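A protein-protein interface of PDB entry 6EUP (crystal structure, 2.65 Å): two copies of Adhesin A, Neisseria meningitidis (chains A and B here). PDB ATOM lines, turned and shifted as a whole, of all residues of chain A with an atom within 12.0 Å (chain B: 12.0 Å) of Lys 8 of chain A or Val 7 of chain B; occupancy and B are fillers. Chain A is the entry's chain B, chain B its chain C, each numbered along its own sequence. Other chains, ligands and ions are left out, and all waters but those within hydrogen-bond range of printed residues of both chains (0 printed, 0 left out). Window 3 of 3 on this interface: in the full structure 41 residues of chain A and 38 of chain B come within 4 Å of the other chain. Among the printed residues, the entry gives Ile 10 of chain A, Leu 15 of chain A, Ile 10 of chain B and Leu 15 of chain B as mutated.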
ATOM      1  N   ASP A   5     -13.137   4.680  19.129  1.00  0.00           N
ATOM      2  CA  ASP A   5     -13.287   3.846  20.321  1.00  0.00           C
ATOM      3  C   ASP A   5     -14.305   2.700  20.117  1.00  0.00           C
ATOM      4  O   ASP A   5     -15.124   2.731  19.187  1.00  0.00           O
ATOM      5  CB  ASP A   5     -13.676   4.700  21.552  1.00  0.00           C
ATOM      6  CG  ASP A   5     -13.019   4.268  22.855  1.00  0.00           C
ATOM      7  OD1 ASP A   5     -13.307   3.142  23.329  1.00  0.00           O
ATOM      8  OD2 ASP A   5     -12.245   5.071  23.420  1.00  0.00           O
ATOM      9  N   ASP A   6     -14.230   1.686  21.000  1.00  0.00           N
ATOM     10  CA  ASP A   6     -15.129   0.536  21.014  1.00  0.00           C
ATOM     11  C   ASP A   6     -16.502   0.969  21.512  1.00  0.00           C
ATOM     12  O   ASP A   6     -17.508   0.432  21.042  1.00  0.00           O
ATOM     13  CB  ASP A   6     -14.560  -0.595  21.885  1.00  0.00           C
ATOM     14  CG  ASP A   6     -14.193  -1.868  21.134  1.00  0.00           C
ATOM     15  OD1 ASP A   6     -14.313  -1.885  19.880  1.00  0.00           O
ATOM     16  OD2 ASP A   6     -13.817  -2.858  21.798  1.00  0.00           O
ATOM     17  N   VAL A   7     -16.543   1.959  22.438  1.00  0.00           N
ATOM     18  CA  VAL A   7     -17.787   2.531  22.981  1.00  0.00           C
ATOM     19  C   VAL A   7     -18.518   3.355  21.920  1.00  0.00           C
ATOM     20  O   VAL A   7     -19.748   3.426  21.965  1.00  0.00           O
ATOM     21  CB  VAL A   7     -17.653   3.296  24.326  1.00  0.00           C
ATOM     22  CG1 VAL A   7     -17.243   2.355  25.448  1.00  0.00           C
ATOM     23  CG2 VAL A   7     -16.694   4.478  24.221  1.00  0.00           C
ATOM     24  N   LYS A   8     -17.769   3.951  20.955  1.00  0.00           N
ATOM     25  CA  LYS A   8     -18.326   4.703  19.829  1.00  0.00           C
ATOM     26  C   LYS A   8     -19.134   3.722  18.981  1.00  0.00           C
ATOM     27  O   LYS A   8     -20.293   3.988  18.675  1.00  0.00           O
ATOM     28  CB  LYS A   8     -17.205   5.345  18.992  1.00  0.00           C
ATOM     29  CG  LYS A   8     -17.660   5.932  17.646  1.00  0.00           C
ATOM     30  CD  LYS A   8     -16.571   6.784  16.964  1.00  0.00           C
ATOM     31  CE  LYS A   8     -15.551   5.996  16.168  1.00  0.00           C
ATOM     32  NZ  LYS A   8     -14.597   6.887  15.454  1.00  0.00           N
ATOM     33  N   LYS A   9     -18.526   2.563  18.663  1.00  0.00           N
ATOM     34  CA  LYS A   9     -19.127   1.499  17.877  1.00  0.00           C
ATOM     35  C   LYS A   9     -20.393   0.941  18.545  1.00  0.00           C
ATOM     36  O   LYS A   9     -21.442   0.943  17.898  1.00  0.00           O
ATOM     37  CB  LYS A   9     -18.093   0.400  17.556  1.00  0.00           C
ATOM     38  CG  LYS A   9     -18.496  -0.483  16.378  1.00  0.00           C
ATOM     39  CD  LYS A   9     -17.307  -1.163  15.708  1.00  0.00           C
ATOM     40  CE  LYS A   9     -17.743  -2.144  14.639  1.00  0.00           C
ATOM     41  NZ  LYS A   9     -18.380  -1.477  13.467  1.00  0.00           N
ATOM     42  N   ILE A  10     -20.316   0.527  19.835  1.00  0.00           N
ATOM     43  CA  ILE A  10     -21.451  -0.012  20.603  1.00  0.00           C
ATOM     44  C   ILE A  10     -22.634   0.978  20.618  1.00  0.00           C
ATOM     45  O   ILE A  10     -23.771   0.561  20.371  1.00  0.00           O
ATOM     46  CB  ILE A  10     -21.016  -0.481  22.025  1.00  0.00           C
ATOM     47  CG1 ILE A  10     -20.030  -1.663  21.946  1.00  0.00           C
ATOM     48  CG2 ILE A  10     -22.214  -0.830  22.931  1.00  0.00           C
ATOM     49  CD1 ILE A  10     -19.039  -1.731  23.103  1.00  0.00           C
ATOM     50  N   ALA A  11     -22.357   2.284  20.850  1.00  0.00           N
ATOM     51  CA  ALA A  11     -23.381   3.336  20.866  1.00  0.00           C
ATOM     52  C   ALA A  11     -24.039   3.535  19.493  1.00  0.00           C
ATOM     53  O   ALA A  11     -25.264   3.676  19.424  1.00  0.00           O
ATOM     54  CB  ALA A  11     -22.801   4.644  21.378  1.00  0.00           C
ATOM     55  N   THR A  12     -23.236   3.510  18.412  1.00  0.00           N
ATOM     56  CA  THR A  12     -23.714   3.659  17.034  1.00  0.00           C
ATOM     57  C   THR A  12     -24.649   2.503  16.643  1.00  0.00           C
ATOM     58  O   THR A  12     -25.738   2.749  16.112  1.00  0.00           O
ATOM     59  CB  THR A  12     -22.546   3.836  16.054  1.00  0.00           C
ATOM     60  OG1 THR A  12     -21.673   4.834  16.562  1.00  0.00           O
ATOM     61  CG2 THR A  12     -23.010   4.274  14.680  1.00  0.00           C
ATOM     62  N   VAL A  13     -24.228   1.254  16.934  1.00  0.00           N
ATOM     63  CA  VAL A  13     -25.009   0.053  16.645  1.00  0.00           C
ATOM     64  C   VAL A  13     -26.328   0.098  17.423  1.00  0.00           C
ATOM     65  O   VAL A  13     -27.366  -0.119  16.821  1.00  0.00           O
ATOM     66  CB  VAL A  13     -24.196  -1.247  16.898  1.00  0.00           C
ATOM     67  CG1 VAL A  13     -25.060  -2.495  16.716  1.00  0.00           C
ATOM     68  CG2 VAL A  13     -22.968  -1.315  15.996  1.00  0.00           C
ATOM     69  N   ALA A  14     -26.281   0.431  18.734  1.00  0.00           N
ATOM     70  CA  ALA A  14     -27.443   0.538  19.625  1.00  0.00           C
ATOM     71  C   ALA A  14     -28.453   1.537  19.095  1.00  0.00           C
ATOM     72  O   ALA A  14     -29.630   1.202  19.019  1.00  0.00           O
ATOM     73  CB  ALA A  14     -27.011   0.932  21.029  1.00  0.00           C
ATOM     74  N   LEU A  15     -28.003   2.731  18.670  1.00  0.00           N
ATOM     75  CA  LEU A  15     -28.892   3.750  18.117  1.00  0.00           C
ATOM     76  C   LEU A  15     -29.606   3.261  16.855  1.00  0.00           C
ATOM     77  O   LEU A  15     -30.834   3.336  16.794  1.00  0.00           O
ATOM     78  CB  LEU A  15     -28.146   5.076  17.875  1.00  0.00           C
ATOM     79  CG  LEU A  15     -29.002   6.275  17.459  1.00  0.00           C
ATOM     80  CD1 LEU A  15     -30.200   6.476  18.391  1.00  0.00           C
ATOM     81  CD2 LEU A  15     -28.176   7.528  17.420  1.00  0.00           C
ATOM     82  N   ALA A  16     -28.840   2.725  15.881  1.00  0.00           N
ATOM     83  CA  ALA A  16     -29.331   2.167  14.624  1.00  0.00           C
ATOM     84  C   ALA A  16     -30.289   0.981  14.894  1.00  0.00           C
ATOM     85  O   ALA A  16     -31.341   0.905  14.256  1.00  0.00           O
ATOM     86  CB  ALA A  16     -28.155   1.716  13.776  1.00  0.00           C
ATOM     87  N   ALA A  17     -29.953   0.092  15.868  1.00  0.00           N
ATOM     88  CA  ALA A  17     -30.795  -1.046  16.247  1.00  0.00           C
ATOM     89  C   ALA A  17     -32.112  -0.557  16.840  1.00  0.00           C
ATOM     90  O   ALA A  17     -33.169  -1.073  16.463  1.00  0.00           O
ATOM     91  CB  ALA A  17     -30.072  -1.959  17.232  1.00  0.00           C
ATOM     92  N   ILE A  37     -27.633  -3.172   9.788  1.00  0.00           N
ATOM     93  CA  ILE A  37     -26.488  -3.532  10.624  1.00  0.00           C
ATOM     94  C   ILE A  37     -25.955  -4.896  10.192  1.00  0.00           C
ATOM     95  O   ILE A  37     -26.577  -5.936  10.443  1.00  0.00           O
ATOM     96  CB  ILE A  37     -26.695  -3.411  12.164  1.00  0.00           C
ATOM     97  CG1 ILE A  37     -27.304  -2.044  12.563  1.00  0.00           C
ATOM     98  CG2 ILE A  37     -25.367  -3.663  12.900  1.00  0.00           C
ATOM     99  CD1 ILE A  37     -28.024  -2.037  13.891  1.00  0.00           C
ATOM    100  N   ASP A  40     -20.775  -7.768  11.036  1.00  0.00           N
ATOM    101  CA  ASP A  40     -19.500  -7.210  11.508  1.00  0.00           C
ATOM    102  C   ASP A  40     -19.707  -5.846  12.232  1.00  0.00           C
ATOM    103  O   ASP A  40     -18.739  -5.101  12.441  1.00  0.00           O
ATOM    104  CB  ASP A  40     -18.504  -7.066  10.333  1.00  0.00           C
ATOM    105  CG  ASP A  40     -18.169  -8.366   9.626  1.00  0.00           C
ATOM    106  OD1 ASP A  40     -19.092  -8.978   9.035  1.00  0.00           O
ATOM    107  OD2 ASP A  40     -16.981  -8.759   9.636  1.00  0.00           O
ATOM    108  N   GLY A  41     -20.959  -5.557  12.609  1.00  0.00           N
ATOM    109  CA  GLY A  41     -21.367  -4.330  13.290  1.00  0.00           C
ATOM    110  C   GLY A  41     -21.255  -3.079  12.440  1.00  0.00           C
ATOM    111  O   GLY A  41     -21.088  -1.976  12.978  1.00  0.00           O
ATOM    112  N   THR A  42     -21.346  -3.244  11.100  1.00  0.00           N
ATOM    113  CA  THR A  42     -21.246  -2.154  10.122  1.00  0.00           C
ATOM    114  C   THR A  42     -22.634  -1.575   9.825  1.00  0.00           C
ATOM    115  O   THR A  42     -23.550  -2.317   9.462  1.00  0.00           O
ATOM    116  CB  THR A  42     -20.503  -2.613   8.844  1.00  0.00           C
ATOM    117  OG1 THR A  42     -19.370  -3.414   9.192  1.00  0.00           O
ATOM    118  CG2 THR A  42     -20.068  -1.445   7.957  1.00  0.00           C
ATOM    119  N   ILE A  43     -22.777  -0.246   9.985  1.00  0.00           N
ATOM    120  CA  ILE A  43     -24.027   0.477   9.743  1.00  0.00           C
ATOM    121  C   ILE A  43     -24.029   1.038   8.329  1.00  0.00           C
ATOM    122  O   ILE A  43     -23.093   1.746   7.946  1.00  0.00           O
ATOM    123  CB  ILE A  43     -24.303   1.540  10.849  1.00  0.00           C
ATOM    124  CG1 ILE A  43     -24.772   0.862  12.137  1.00  0.00           C
ATOM    125  CG2 ILE A  43     -25.308   2.611  10.414  1.00  0.00           C
ATOM    126  CD1 ILE A  43     -23.791   0.879  13.176  1.00  0.00           C
ATOM    127  N   ASP B   5     -19.344  14.779  25.139  1.00  0.00           N
ATOM    128  CA  ASP B   5     -18.950  14.126  23.892  1.00  0.00           C
ATOM    129  C   ASP B   5     -20.171  13.787  23.015  1.00  0.00           C
ATOM    130  O   ASP B   5     -21.313  13.759  23.499  1.00  0.00           O
ATOM    131  CB  ASP B   5     -18.109  12.853  24.163  1.00  0.00           C
ATOM    132  CG  ASP B   5     -16.974  12.646  23.174  1.00  0.00           C
ATOM    133  OD1 ASP B   5     -15.846  13.112  23.455  1.00  0.00           O
ATOM    134  OD2 ASP B   5     -17.218  12.048  22.105  1.00  0.00           O
ATOM    135  N   ASP B   6     -19.908  13.538  21.712  1.00  0.00           N
ATOM    136  CA  ASP B   6     -20.899  13.158  20.703  1.00  0.00           C
ATOM    137  C   ASP B   6     -21.354  11.725  20.984  1.00  0.00           C
ATOM    138  O   ASP B   6     -22.525  11.415  20.767  1.00  0.00           O
ATOM    139  CB  ASP B   6     -20.315  13.260  19.271  1.00  0.00           C
ATOM    140  CG  ASP B   6     -19.187  14.273  19.064  1.00  0.00           C
ATOM    141  OD1 ASP B   6     -19.330  15.426  19.534  1.00  0.00           O
ATOM    142  OD2 ASP B   6     -18.149  13.902  18.450  1.00  0.00           O
ATOM    143  N   VAL B   7     -20.433  10.857  21.494  1.00  0.00           N
ATOM    144  CA  VAL B   7     -20.721   9.460  21.857  1.00  0.00           C
ATOM    145  C   VAL B   7     -21.612   9.393  23.096  1.00  0.00           C
ATOM    146  O   VAL B   7     -22.383   8.441  23.220  1.00  0.00           O
ATOM    147  CB  VAL B   7     -19.488   8.524  21.970  1.00  0.00           C
ATOM    148  CG1 VAL B   7     -18.813   8.342  20.620  1.00  0.00           C
ATOM    149  CG2 VAL B   7     -18.492   9.009  23.022  1.00  0.00           C
ATOM    150  N   LYS B   8     -21.525  10.409  23.994  1.00  0.00           N
ATOM    151  CA  LYS B   8     -22.368  10.520  25.186  1.00  0.00           C
ATOM    152  C   LYS B   8     -23.807  10.696  24.711  1.00  0.00           C
ATOM    153  O   LYS B   8     -24.692   9.964  25.149  1.00  0.00           O
ATOM    154  CB  LYS B   8     -21.932  11.713  26.058  1.00  0.00           C
ATOM    155  CG  LYS B   8     -22.918  12.083  27.182  1.00  0.00           C
ATOM    156  CD  LYS B   8     -22.346  13.110  28.177  1.00  0.00           C
ATOM    157  CE  LYS B   8     -22.433  14.557  27.734  1.00  0.00           C
ATOM    158  NZ  LYS B   8     -21.916  15.487  28.777  1.00  0.00           N
ATOM    159  N   LYS B   9     -24.010  11.630  23.763  1.00  0.00           N
ATOM    160  CA  LYS B   9     -25.302  11.946  23.173  1.00  0.00           C
ATOM    161  C   LYS B   9     -25.914  10.733  22.462  1.00  0.00           C
ATOM    162  O   LYS B   9     -27.036  10.369  22.810  1.00  0.00           O
ATOM    163  CB  LYS B   9     -25.202  13.182  22.260  1.00  0.00           C
ATOM    164  CG  LYS B   9     -26.550  13.852  22.017  1.00  0.00           C
ATOM    165  CD  LYS B   9     -26.422  15.303  21.563  1.00  0.00           C
ATOM    166  CE  LYS B   9     -27.747  15.882  21.113  1.00  0.00           C
ATOM    167  NZ  LYS B   9     -28.714  16.012  22.235  1.00  0.00           N
ATOM    168  N   ILE B  10     -25.168  10.079  21.534  1.00  0.00           N
ATOM    169  CA  ILE B  10     -25.616   8.892  20.789  1.00  0.00           C
ATOM    170  C   ILE B  10     -26.055   7.761  21.749  1.00  0.00           C
ATOM    171  O   ILE B  10     -27.119   7.173  21.542  1.00  0.00           O
ATOM    172  CB  ILE B  10     -24.559   8.437  19.738  1.00  0.00           C
ATOM    173  CG1 ILE B  10     -24.367   9.498  18.643  1.00  0.00           C
ATOM    174  CG2 ILE B  10     -24.881   7.068  19.119  1.00  0.00           C
ATOM    175  CD1 ILE B  10     -22.968   9.510  18.028  1.00  0.00           C
ATOM    176  N   ALA B  11     -25.269   7.503  22.815  1.00  0.00           N
ATOM    177  CA  ALA B  11     -25.581   6.476  23.815  1.00  0.00           C
ATOM    178  C   ALA B  11     -26.844   6.807  24.615  1.00  0.00           C
ATOM    179  O   ALA B  11     -27.662   5.910  24.856  1.00  0.00           O
ATOM    180  CB  ALA B  11     -24.398   6.254  24.747  1.00  0.00           C
ATOM    181  N   THR B  12     -27.019   8.093  24.993  1.00  0.00           N
ATOM    182  CA  THR B  12     -28.188   8.569  25.750  1.00  0.00           C
ATOM    183  C   THR B  12     -29.475   8.412  24.927  1.00  0.00           C
ATOM    184  O   THR B  12     -30.469   7.888  25.442  1.00  0.00           O
ATOM    185  CB  THR B  12     -27.971  10.003  26.253  1.00  0.00           C
ATOM    186  OG1 THR B  12     -26.706  10.074  26.892  1.00  0.00           O
ATOM    187  CG2 THR B  12     -29.017  10.431  27.257  1.00  0.00           C
ATOM    188  N   VAL B  13     -29.434   8.840  23.643  1.00  0.00           N
ATOM    189  CA  VAL B  13     -30.560   8.745  22.720  1.00  0.00           C
ATOM    190  C   VAL B  13     -30.925   7.268  22.509  1.00  0.00           C
ATOM    191  O   VAL B  13     -32.100   6.936  22.618  1.00  0.00           O
ATOM    192  CB  VAL B  13     -30.299   9.500  21.391  1.00  0.00           C
ATOM    193  CG1 VAL B  13     -31.438   9.290  20.398  1.00  0.00           C
ATOM    194  CG2 VAL B  13     -30.091  10.990  21.633  1.00  0.00           C
ATOM    195  N   ALA B  14     -29.918   6.393  22.261  1.00  0.00           N
ATOM    196  CA  ALA B  14     -30.088   4.953  22.048  1.00  0.00           C
ATOM    197  C   ALA B  14     -30.773   4.296  23.233  1.00  0.00           C
ATOM    198  O   ALA B  14     -31.736   3.559  23.026  1.00  0.00           O
ATOM    199  CB  ALA B  14     -28.750   4.286  21.788  1.00  0.00           C
ATOM    200  N   LEU B  15     -30.332   4.604  24.472  1.00  0.00           N
ATOM    201  CA  LEU B  15     -30.948   4.046  25.675  1.00  0.00           C
ATOM    202  C   LEU B  15     -32.417   4.445  25.793  1.00  0.00           C
ATOM    203  O   LEU B  15     -33.257   3.568  25.947  1.00  0.00           O
ATOM    204  CB  LEU B  15     -30.155   4.416  26.939  1.00  0.00           C
ATOM    205  CG  LEU B  15     -30.632   3.776  28.254  1.00  0.00           C
ATOM    206  CD1 LEU B  15     -30.804   2.248  28.128  1.00  0.00           C
ATOM    207  CD2 LEU B  15     -29.704   4.117  29.381  1.00  0.00           C
ATOM    208  N   ALA B  16     -32.718   5.753  25.668  1.00  0.00           N
ATOM    209  CA  ALA B  16     -34.058   6.327  25.717  1.00  0.00           C
ATOM    210  C   ALA B  16     -34.940   5.741  24.596  1.00  0.00           C
ATOM    211  O   ALA B  16     -36.088   5.392  24.862  1.00  0.00           O
ATOM    212  CB  ALA B  16     -33.970   7.842  25.604  1.00  0.00           C
ATOM    213  N   GLY B  41     -32.432  15.627  19.061  1.00  0.00           N
ATOM    214  CA  GLY B  41     -31.829  14.608  19.915  1.00  0.00           C
ATOM    215  C   GLY B  41     -31.869  14.931  21.395  1.00  0.00           C
ATOM    216  O   GLY B  41     -31.022  14.447  22.154  1.00  0.00           O
ATOM    217  N   ILE B  43     -33.476  14.691  25.092  1.00  0.00           N
ATOM    218  CA  ILE B  43     -34.219  13.752  25.934  1.00  0.00           C
ATOM    219  C   ILE B  43     -34.932  14.509  27.043  1.00  0.00           C
ATOM    220  O   ILE B  43     -34.296  15.264  27.782  1.00  0.00           O
ATOM    221  CB  ILE B  43     -33.316  12.587  26.442  1.00  0.00           C
ATOM    222  CG1 ILE B  43     -33.044  11.587  25.320  1.00  0.00           C
ATOM    223  CG2 ILE B  43     -33.898  11.863  27.658  1.00  0.00           C
ATOM    224  CD1 ILE B  43     -31.705  11.639  24.843  1.00  0.00           C
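No residue of chain B comes within 4 Å of Asp 6 of chain A.
No residue of chain B comes within 4 Å of Val 7 of chain A.
Lys 8 of chain A touches just one residue of chain B: Val 7 (3.8 Å).
No residue of chain B comes within 4 Å of Ile 10 of chain A.
Ala 11 of chain A touches just one residue of chain B: Ile 10 (3.4 Å).
Gly 41 of chain A touches none of the printed residues of chain B.
No residue of chain A comes within 4 Å of Asp 5 of chain B.
Val 7 of chain B touches just one residue of chain A: Lys 8.
No residue of chain A comes within 4 Å of Ala 11 of chain B.
Of the printed residues of chain A, Val 13 of chain B touches Leu 15 (3.7 Å).
Printed residues of chain A within 4 Å of Ala 14 of chain B: Ala 14 and Leu 15.
Gly 41 of chain B touches none of the printed residues of chain A.
The nearest residue of chain B that does not touch Lys 8 of chain A is Ile 10 of chain B (5.5 Å).
The nearest residue of chain A that does not touch Val 7 of chain B is Ala 11 of chain A (4.2 Å).
The nearest printed residue of chain B that does not touch Ala 14 of chain A is Leu 15 of chain B (6.0 Å).
Thr 12 of chain A touches Ile 10 of chain B, but with the chains exchanged Ile 10 of chain A does not touch Thr 12 of chain B (9.4 Å).
Ala 14 of chain B touches its own counterpart, Ala 14 of chain A.
Leu 15 of chain A touches Val 13 of chain B, but with the chains exchanged Val 13 of chain A does not touch Leu 15 of chain B (9.3 Å).
Leu 15 of chain A touches Ala 14 of chain B, but with the chains exchanged Ala 14 of chain A does not touch Leu 15 of chain B (6.0 Å).
Of the 7 pairs that touch across the chains among the printed residues, 1 has its exchanged pair printed and touching as well.
Lys 8 of chain A touches Val 7 of chain B (CA to CG1, 3.8 Å).
Ala 11 of chain A touches Ile 10 of chain B (O to CG2, 3.4 Å).
Thr 12 of chain A touches Ile 10 of chain B (N to CG2, 3.98 Å).
Ala 14 of chain A touches Ala 14 of chain B.
Leu 15 of chain A touches Ile 10 of chain B (CD2 to CG2, 3.7 Å).
Val 13 of chain B touches Leu 15 of chain A.
CB of Ala 14 of chain B touches N of Leu 15 of chain A (3.6 Å).
The side-chain hydroxyl of Thr 12 of chain A is in hydrogen-bond range of the backbone carbonyl oxygen of Lys 8 of chain A.
The side-chain carboxylate of Asp 5 of chain B lies close to the backbone NH of Val 7 of chain B (3.5 Å).
Printed residues of chain A that touch a printed residue of chain B: Lys 8, Ala 11, Thr 12, Ala 14 and Leu 15.
Hydrophobic or aromatic side chains of chain B that line the printed part of chain A: Val 7, Ile 10, Val 13 and Ala 14.
Among the printed residues, 7 pairs touch across the chains.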
